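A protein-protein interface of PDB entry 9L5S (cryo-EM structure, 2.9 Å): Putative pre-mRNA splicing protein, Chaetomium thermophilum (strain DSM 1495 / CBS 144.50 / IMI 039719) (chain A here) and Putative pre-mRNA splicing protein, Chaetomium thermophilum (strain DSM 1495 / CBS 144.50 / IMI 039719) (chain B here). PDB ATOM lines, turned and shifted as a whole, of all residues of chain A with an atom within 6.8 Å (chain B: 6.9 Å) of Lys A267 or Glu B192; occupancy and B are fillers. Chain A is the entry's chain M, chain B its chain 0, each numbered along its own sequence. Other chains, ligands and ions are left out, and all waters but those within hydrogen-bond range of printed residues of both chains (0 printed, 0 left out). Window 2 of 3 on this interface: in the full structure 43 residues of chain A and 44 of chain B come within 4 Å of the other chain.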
ATOM      1  N   ARG A 257     -14.389  -4.050  12.137  1.00  0.00           N
ATOM      2  CA  ARG A 257     -13.960  -2.716  11.724  1.00  0.00           C
ATOM      3  C   ARG A 257     -14.881  -2.121  10.666  1.00  0.00           C
ATOM      4  O   ARG A 257     -15.280  -0.956  10.778  1.00  0.00           O
ATOM      5  CB  ARG A 257     -12.519  -2.756  11.219  1.00  0.00           C
ATOM      6  CG  ARG A 257     -11.943  -1.382  10.913  1.00  0.00           C
ATOM      7  CD  ARG A 257     -10.451  -1.445  10.637  1.00  0.00           C
ATOM      8  NE  ARG A 257      -9.682  -1.639  11.860  1.00  0.00           N
ATOM      9  CZ  ARG A 257      -9.200  -0.652  12.604  1.00  0.00           C
ATOM     10  NH1 ARG A 257      -9.393   0.616  12.280  1.00  0.00           N
ATOM     11  NH2 ARG A 257      -8.506  -0.945  13.700  1.00  0.00           N
ATOM     12  N   LYS A 265     -15.656   7.524  12.182  1.00  0.00           N
ATOM     13  CA  LYS A 265     -14.229   7.261  12.052  1.00  0.00           C
ATOM     14  C   LYS A 265     -13.709   6.611  13.328  1.00  0.00           C
ATOM     15  O   LYS A 265     -13.794   7.200  14.412  1.00  0.00           O
ATOM     16  CB  LYS A 265     -13.475   8.557  11.759  1.00  0.00           C
ATOM     17  CG  LYS A 265     -12.004   8.361  11.440  1.00  0.00           C
ATOM     18  CD  LYS A 265     -11.409   9.602  10.799  1.00  0.00           C
ATOM     19  CE  LYS A 265      -9.891   9.545  10.791  1.00  0.00           C
ATOM     20  NZ  LYS A 265      -9.288  10.842  11.205  1.00  0.00           N
ATOM     21  N   ILE A 266     -13.164   5.406  13.200  1.00  0.00           N
ATOM     22  CA  ILE A 266     -12.670   4.634  14.334  1.00  0.00           C
ATOM     23  C   ILE A 266     -11.187   4.927  14.505  1.00  0.00           C
ATOM     24  O   ILE A 266     -10.389   4.684  13.592  1.00  0.00           O
ATOM     25  CB  ILE A 266     -12.913   3.130  14.139  1.00  0.00           C
ATOM     26  CG1 ILE A 266     -14.318   2.880  13.593  1.00  0.00           C
ATOM     27  CG2 ILE A 266     -12.707   2.385  15.446  1.00  0.00           C
ATOM     28  CD1 ILE A 266     -14.512   1.485  13.047  1.00  0.00           C
ATOM     29  N   LYS A 267     -10.816   5.453  15.675  1.00  0.00           N
ATOM     30  CA  LYS A 267      -9.404   5.687  15.958  1.00  0.00           C
ATOM     31  C   LYS A 267      -8.668   4.378  16.221  1.00  0.00           C
ATOM     32  O   LYS A 267      -7.546   4.183  15.741  1.00  0.00           O
ATOM     33  CB  LYS A 267      -9.257   6.639  17.146  1.00  0.00           C
ATOM     34  CG  LYS A 267      -7.818   6.904  17.562  1.00  0.00           C
ATOM     35  CD  LYS A 267      -7.747   7.881  18.724  1.00  0.00           C
ATOM     36  CE  LYS A 267      -6.310   8.102  19.169  1.00  0.00           C
ATOM     37  NZ  LYS A 267      -6.210   9.131  20.241  1.00  0.00           N
ATOM     38  N   SER A 268      -9.285   3.465  16.969  1.00  0.00           N
ATOM     39  CA  SER A 268      -8.630   2.216  17.328  1.00  0.00           C
ATOM     40  C   SER A 268      -9.666   1.124  17.546  1.00  0.00           C
ATOM     41  O   SER A 268     -10.786   1.387  17.994  1.00  0.00           O
ATOM     42  CB  SER A 268      -7.773   2.376  18.591  1.00  0.00           C
ATOM     43  OG  SER A 268      -6.634   3.179  18.339  1.00  0.00           O
ATOM     44  N   LEU A 269      -9.271  -0.110  17.242  1.00  0.00           N
ATOM     45  CA  LEU A 269     -10.103  -1.287  17.486  1.00  0.00           C
ATOM     46  C   LEU A 269      -9.193  -2.408  17.967  1.00  0.00           C
ATOM     47  O   LEU A 269      -8.392  -2.937  17.191  1.00  0.00           O
ATOM     48  CB  LEU A 269     -10.870  -1.703  16.231  1.00  0.00           C
ATOM     49  CG  LEU A 269     -11.543  -3.080  16.256  1.00  0.00           C
ATOM     50  CD1 LEU A 269     -12.578  -3.173  17.366  1.00  0.00           C
ATOM     51  CD2 LEU A 269     -12.172  -3.394  14.913  1.00  0.00           C
ATOM     52  N   VAL A 270      -9.313  -2.765  19.242  1.00  0.00           N
ATOM     53  CA  VAL A 270      -8.516  -3.825  19.848  1.00  0.00           C
ATOM     54  C   VAL A 270      -9.406  -5.043  20.030  1.00  0.00           C
ATOM     55  O   VAL A 270     -10.378  -4.998  20.790  1.00  0.00           O
ATOM     56  CB  VAL A 270      -7.924  -3.382  21.195  1.00  0.00           C
ATOM     57  CG1 VAL A 270      -7.152  -4.526  21.826  1.00  0.00           C
ATOM     58  CG2 VAL A 270      -7.044  -2.160  21.019  1.00  0.00           C
ATOM     59  N   VAL A 280     -13.469  -0.501  21.252  1.00  0.00           N
ATOM     60  CA  VAL A 280     -13.596   0.406  20.116  1.00  0.00           C
ATOM     61  C   VAL A 280     -13.409   1.825  20.630  1.00  0.00           C
ATOM     62  O   VAL A 280     -14.178   2.287  21.482  1.00  0.00           O
ATOM     63  CB  VAL A 280     -14.954   0.257  19.415  1.00  0.00           C
ATOM     64  CG1 VAL A 280     -15.007   1.130  18.173  1.00  0.00           C
ATOM     65  CG2 VAL A 280     -15.216  -1.194  19.068  1.00  0.00           C
ATOM     66  N   ASN A 281     -12.394   2.517  20.119  1.00  0.00           N
ATOM     67  CA  ASN A 281     -12.135   3.907  20.467  1.00  0.00           C
ATOM     68  C   ASN A 281     -12.363   4.758  19.228  1.00  0.00           C
ATOM     69  O   ASN A 281     -11.626   4.635  18.245  1.00  0.00           O
ATOM     70  CB  ASN A 281     -10.713   4.088  20.998  1.00  0.00           C
ATOM     71  CG  ASN A 281     -10.497   3.400  22.331  1.00  0.00           C
ATOM     72  OD1 ASN A 281     -11.068   3.796  23.347  1.00  0.00           O
ATOM     73  ND2 ASN A 281      -9.667   2.362  22.334  1.00  0.00           N
ATOM     74  N   TYR A 282     -13.386   5.606  19.275  1.00  0.00           N
ATOM     75  CA  TYR A 282     -13.725   6.480  18.167  1.00  0.00           C
ATOM     76  C   TYR A 282     -12.912   7.771  18.253  1.00  0.00           C
ATOM     77  O   TYR A 282     -12.099   7.967  19.159  1.00  0.00           O
ATOM     78  CB  TYR A 282     -15.224   6.778  18.167  1.00  0.00           C
ATOM     79  CG  TYR A 282     -16.050   5.842  17.312  1.00  0.00           C
ATOM     80  CD1 TYR A 282     -16.384   6.176  16.005  1.00  0.00           C
ATOM     81  CD2 TYR A 282     -16.503   4.630  17.816  1.00  0.00           C
ATOM     82  CE1 TYR A 282     -17.141   5.325  15.222  1.00  0.00           C
ATOM     83  CE2 TYR A 282     -17.262   3.772  17.040  1.00  0.00           C
ATOM     84  CZ  TYR A 282     -17.577   4.124  15.744  1.00  0.00           C
ATOM     85  OH  TYR A 282     -18.331   3.274  14.968  1.00  0.00           O
ATOM     86  N   GLU A 283     -13.136   8.667  17.295  1.00  0.00           N
ATOM     87  CA  GLU A 283     -12.563  10.005  17.344  1.00  0.00           C
ATOM     88  C   GLU A 283     -13.574  11.061  17.764  1.00  0.00           C
ATOM     89  O   GLU A 283     -13.199  12.043  18.413  1.00  0.00           O
ATOM     90  CB  GLU A 283     -11.968  10.383  15.983  1.00  0.00           C
ATOM     91  CG  GLU A 283     -10.979  11.539  16.037  1.00  0.00           C
ATOM     92  CD  GLU A 283     -10.183  11.688  14.756  1.00  0.00           C
ATOM     93  OE1 GLU A 283     -10.408  10.895  13.819  1.00  0.00           O
ATOM     94  OE2 GLU A 283      -9.331  12.599  14.687  1.00  0.00           O
ATOM     95  N   PRO A 313     -11.456   3.030  28.645  1.00  0.00           N
ATOM     96  CA  PRO A 313     -10.475   2.031  28.190  1.00  0.00           C
ATOM     97  C   PRO A 313      -9.540   1.523  29.278  1.00  0.00           C
ATOM     98  O   PRO A 313      -8.738   2.281  29.831  1.00  0.00           O
ATOM     99  CB  PRO A 313      -9.693   2.779  27.102  1.00  0.00           C
ATOM    100  CG  PRO A 313      -9.915   4.228  27.390  1.00  0.00           C
ATOM    101  CD  PRO A 313     -11.305   4.311  27.933  1.00  0.00           C
ATOM    102  N   ASP B 188       0.890   0.368  30.001  1.00  0.00           N
ATOM    103  CA  ASP B 188      -0.407  -0.280  30.145  1.00  0.00           C
ATOM    104  C   ASP B 188      -1.319  -0.117  28.933  1.00  0.00           C
ATOM    105  O   ASP B 188      -2.292  -0.866  28.809  1.00  0.00           O
ATOM    106  CB  ASP B 188      -1.114   0.226  31.415  1.00  0.00           C
ATOM    107  CG  ASP B 188      -1.416   1.727  31.388  1.00  0.00           C
ATOM    108  OD1 ASP B 188      -1.057   2.432  30.419  1.00  0.00           O
ATOM    109  OD2 ASP B 188      -2.025   2.209  32.367  1.00  0.00           O
ATOM    110  N   ASP B 189      -1.026   0.828  28.043  1.00  0.00           N
ATOM    111  CA  ASP B 189      -1.844   1.088  26.859  1.00  0.00           C
ATOM    112  C   ASP B 189      -1.192   0.566  25.586  1.00  0.00           C
ATOM    113  O   ASP B 189      -1.221   1.235  24.548  1.00  0.00           O
ATOM    114  CB  ASP B 189      -2.140   2.580  26.740  1.00  0.00           C
ATOM    115  CG  ASP B 189      -0.898   3.435  26.894  1.00  0.00           C
ATOM    116  OD1 ASP B 189       0.152   2.891  27.297  1.00  0.00           O
ATOM    117  OD2 ASP B 189      -0.972   4.650  26.616  1.00  0.00           O
ATOM    118  N   ILE B 190      -0.570  -0.616  25.652  1.00  0.00           N
ATOM    119  CA  ILE B 190       0.096  -1.192  24.486  1.00  0.00           C
ATOM    120  C   ILE B 190      -0.913  -1.532  23.396  1.00  0.00           C
ATOM    121  O   ILE B 190      -0.681  -1.259  22.211  1.00  0.00           O
ATOM    122  CB  ILE B 190       0.911  -2.433  24.897  1.00  0.00           C
ATOM    123  CG1 ILE B 190       1.870  -2.090  26.036  1.00  0.00           C
ATOM    124  CG2 ILE B 190       1.673  -2.998  23.703  1.00  0.00           C
ATOM    125  CD1 ILE B 190       3.039  -1.251  25.605  1.00  0.00           C
ATOM    126  N   GLU B 191      -2.047  -2.125  23.784  1.00  0.00           N
ATOM    127  CA  GLU B 191      -2.987  -2.687  22.815  1.00  0.00           C
ATOM    128  C   GLU B 191      -3.595  -1.612  21.922  1.00  0.00           C
ATOM    129  O   GLU B 191      -3.710  -1.801  20.705  1.00  0.00           O
ATOM    130  CB  GLU B 191      -4.084  -3.453  23.550  1.00  0.00           C
ATOM    131  CG  GLU B 191      -3.641  -4.789  24.123  1.00  0.00           C
ATOM    132  CD  GLU B 191      -3.203  -4.686  25.572  1.00  0.00           C
ATOM    133  OE1 GLU B 191      -2.929  -3.559  26.035  1.00  0.00           O
ATOM    134  OE2 GLU B 191      -3.135  -5.733  26.248  1.00  0.00           O
ATOM    135  N   GLU B 192      -3.975  -0.472  22.508  1.00  0.00           N
ATOM    136  CA  GLU B 192      -4.592   0.602  21.733  1.00  0.00           C
ATOM    137  C   GLU B 192      -3.619   1.193  20.720  1.00  0.00           C
ATOM    138  O   GLU B 192      -3.983   1.411  19.559  1.00  0.00           O
ATOM    139  CB  GLU B 192      -5.116   1.686  22.675  1.00  0.00           C
ATOM    140  CG  GLU B 192      -6.105   2.654  22.038  1.00  0.00           C
ATOM    141  CD  GLU B 192      -5.433   3.881  21.452  1.00  0.00           C
ATOM    142  OE1 GLU B 192      -4.360   4.272  21.959  1.00  0.00           O
ATOM    143  OE2 GLU B 192      -5.976   4.452  20.483  1.00  0.00           O
ATOM    144  N   ILE B 193      -2.372   1.438  21.129  1.00  0.00           N
ATOM    145  CA  ILE B 193      -1.417   2.056  20.216  1.00  0.00           C
ATOM    146  C   ILE B 193      -0.952   1.063  19.152  1.00  0.00           C
ATOM    147  O   ILE B 193      -0.670   1.457  18.011  1.00  0.00           O
ATOM    148  CB  ILE B 193      -0.250   2.685  21.009  1.00  0.00           C
ATOM    149  CG1 ILE B 193       0.722   1.631  21.552  1.00  0.00           C
ATOM    150  CG2 ILE B 193      -0.801   3.512  22.160  1.00  0.00           C
ATOM    151  CD1 ILE B 193       1.819   2.198  22.432  1.00  0.00           C
ATOM    152  N   VAL B 194      -0.895  -0.233  19.483  1.00  0.00           N
ATOM    153  CA  VAL B 194      -0.578  -1.244  18.476  1.00  0.00           C
ATOM    154  C   VAL B 194      -1.703  -1.344  17.452  1.00  0.00           C
ATOM    155  O   VAL B 194      -1.456  -1.362  16.241  1.00  0.00           O
ATOM    156  CB  VAL B 194      -0.282  -2.601  19.141  1.00  0.00           C
ATOM    157  CG1 VAL B 194      -0.237  -3.709  18.107  1.00  0.00           C
ATOM    158  CG2 VAL B 194       1.059  -2.547  19.850  1.00  0.00           C
ATOM    159  N   ALA B 195      -2.955  -1.372  17.917  1.00  0.00           N
ATOM    160  CA  ALA B 195      -4.077  -1.449  16.988  1.00  0.00           C
ATOM    161  C   ALA B 195      -4.230  -0.172  16.170  1.00  0.00           C
ATOM    162  O   ALA B 195      -4.760  -0.218  15.054  1.00  0.00           O
ATOM    163  CB  ALA B 195      -5.366  -1.750  17.745  1.00  0.00           C
ATOM    164  N   ARG B 196      -3.786   0.969  16.700  1.00  0.00           N
ATOM    165  CA  ARG B 196      -3.824   2.197  15.914  1.00  0.00           C
ATOM    166  C   ARG B 196      -2.727   2.218  14.857  1.00  0.00           C
ATOM    167  O   ARG B 196      -2.973   2.614  13.711  1.00  0.00           O
ATOM    168  CB  ARG B 196      -3.714   3.418  16.825  1.00  0.00           C
ATOM    169  CG  ARG B 196      -3.916   4.739  16.093  1.00  0.00           C
ATOM    170  CD  ARG B 196      -3.381   5.923  16.881  1.00  0.00           C
ATOM    171  NE  ARG B 196      -3.541   5.746  18.319  1.00  0.00           N
ATOM    172  CZ  ARG B 196      -2.552   5.822  19.199  1.00  0.00           C
ATOM    173  NH1 ARG B 196      -1.307   6.063  18.822  1.00  0.00           N
ATOM    174  NH2 ARG B 196      -2.820   5.654  20.491  1.00  0.00           N
ATOM    175  N   HIS B 197      -1.511   1.797  15.213  1.00  0.00           N
ATOM    176  CA  HIS B 197      -0.380   1.942  14.304  1.00  0.00           C
ATOM    177  C   HIS B 197      -0.120   0.723  13.428  1.00  0.00           C
ATOM    178  O   HIS B 197       0.464   0.877  12.350  1.00  0.00           O
ATOM    179  CB  HIS B 197       0.886   2.298  15.091  1.00  0.00           C
ATOM    180  CG  HIS B 197       0.954   3.741  15.483  1.00  0.00           C
ATOM    181  ND1 HIS B 197       1.885   4.233  16.371  1.00  0.00           N
ATOM    182  CD2 HIS B 197       0.199   4.799  15.104  1.00  0.00           C
ATOM    183  CE1 HIS B 197       1.701   5.533  16.522  1.00  0.00           C
ATOM    184  NE2 HIS B 197       0.684   5.901  15.764  1.00  0.00           N
ATOM    185  N   ALA B 199      -2.282  -0.727  11.601  1.00  0.00           N
ATOM    186  CA  ALA B 199      -3.552  -0.772  10.883  1.00  0.00           C
ATOM    187  C   ALA B 199      -3.550  -0.057   9.541  1.00  0.00           C
ATOM    188  O   ALA B 199      -4.468  -0.292   8.748  1.00  0.00           O
ATOM    189  CB  ALA B 199      -4.676  -0.186  11.745  1.00  0.00           C
ATOM    190  N   VAL B 209      -1.523  -9.464  21.576  1.00  0.00           N
ATOM    191  CA  VAL B 209      -0.459  -8.662  22.243  1.00  0.00           C
ATOM    192  C   VAL B 209      -0.027  -9.391  23.511  1.00  0.00           C
ATOM    193  O   VAL B 209      -0.777  -9.330  24.501  1.00  0.00           O
ATOM    194  CB  VAL B 209      -0.922  -7.230  22.563  1.00  0.00           C
ATOM    195  CG1 VAL B 209       0.205  -6.397  23.149  1.00  0.00           C
ATOM    196  CG2 VAL B 209      -1.511  -6.540  21.344  1.00  0.00           C
ATOM    197  N   ASP B 239       5.433   5.096  20.220  1.00  0.00           N
ATOM    198  CA  ASP B 239       5.040   6.347  20.860  1.00  0.00           C
ATOM    199  C   ASP B 239       6.253   7.082  21.411  1.00  0.00           C
ATOM    200  O   ASP B 239       6.283   8.316  21.437  1.00  0.00           O
ATOM    201  CB  ASP B 239       4.028   6.094  21.977  1.00  0.00           C
ATOM    202  CG  ASP B 239       2.597   6.202  21.499  1.00  0.00           C
ATOM    203  OD1 ASP B 239       2.347   6.944  20.524  1.00  0.00           O
ATOM    204  OD2 ASP B 239       1.720   5.558  22.106  1.00  0.00           O
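OG of Ser A268 is in hydrogen-bond range of OE2 of Glu B192 (2.6 Å).
O of Ser A268 lies within hydrogen-bond range of N of Asn A281, 2.9 Å away. The side-chain carboxylate (OE1) of Glu B192 is in salt-bridge range of the guanidinium group (NH2) of Arg B196, 2.5 Å away. The backbone NH (N) of Lys A267 sits at hydrogen-bond distance from the backbone carbonyl oxygen (O) of Asn A281 (2.8 Å).
Glu B192 touches Lys A267. CG of Arg B196 touches O of Lys A267, 3.7 Å away. CB of Arg B196 touches OG of Ser A268 (3.3 Å). O of Leu A269 touches CB of Ala B195, at 3.3 Å. O of Glu B191 touches CG2 of Val A270, 3.4 Å away. Val A270 touches Glu B192. CG2 of Val A270 touches CB of Ala B195 (3.7 Å). Glu B192 touches Asn A281 (CG to ND2, 3.6 Å).
Lys A267 touches two residues of chain B. Glu B192 touches just these residues of chain A: Lys A267 (3.9 Å), Ser A268 (2.6 Å), Val A270 (3.8 Å) and Asn A281 (3.6 Å). Printed residues of chain B within 4 Å of Asn A281: Glu B192 (3.6 Å). Printed residues of chain A within 4 Å of Arg B196: Lys A267 (3.7 Å) and Ser A268 (3.3 Å). Of the printed residues of chain A, Ala B195 touches Leu A269 (3.3 Å) and Val A270 (3.7 Å). Val A280 touches none of the printed residues of chain B. Ala B199 touches none of the printed residues of chain A. The nearest residue of chain B that does not touch Lys A267 is Ala B195 (5.3 Å). The nearest residue of chain A that does not touch Glu B192 is Leu A269 (6.0 Å).
Hydrophobic or aromatic side chains of chain B within 4 Å of the printed part of chain A: Ala B195. Along chain A the printed residues that touch a printed residue of chain B span positions 267 to 281. Among the printed residues, no Asp or Glu carboxylate lies within 4 Å of a Lys or Arg side-chain nitrogen of the other chain.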
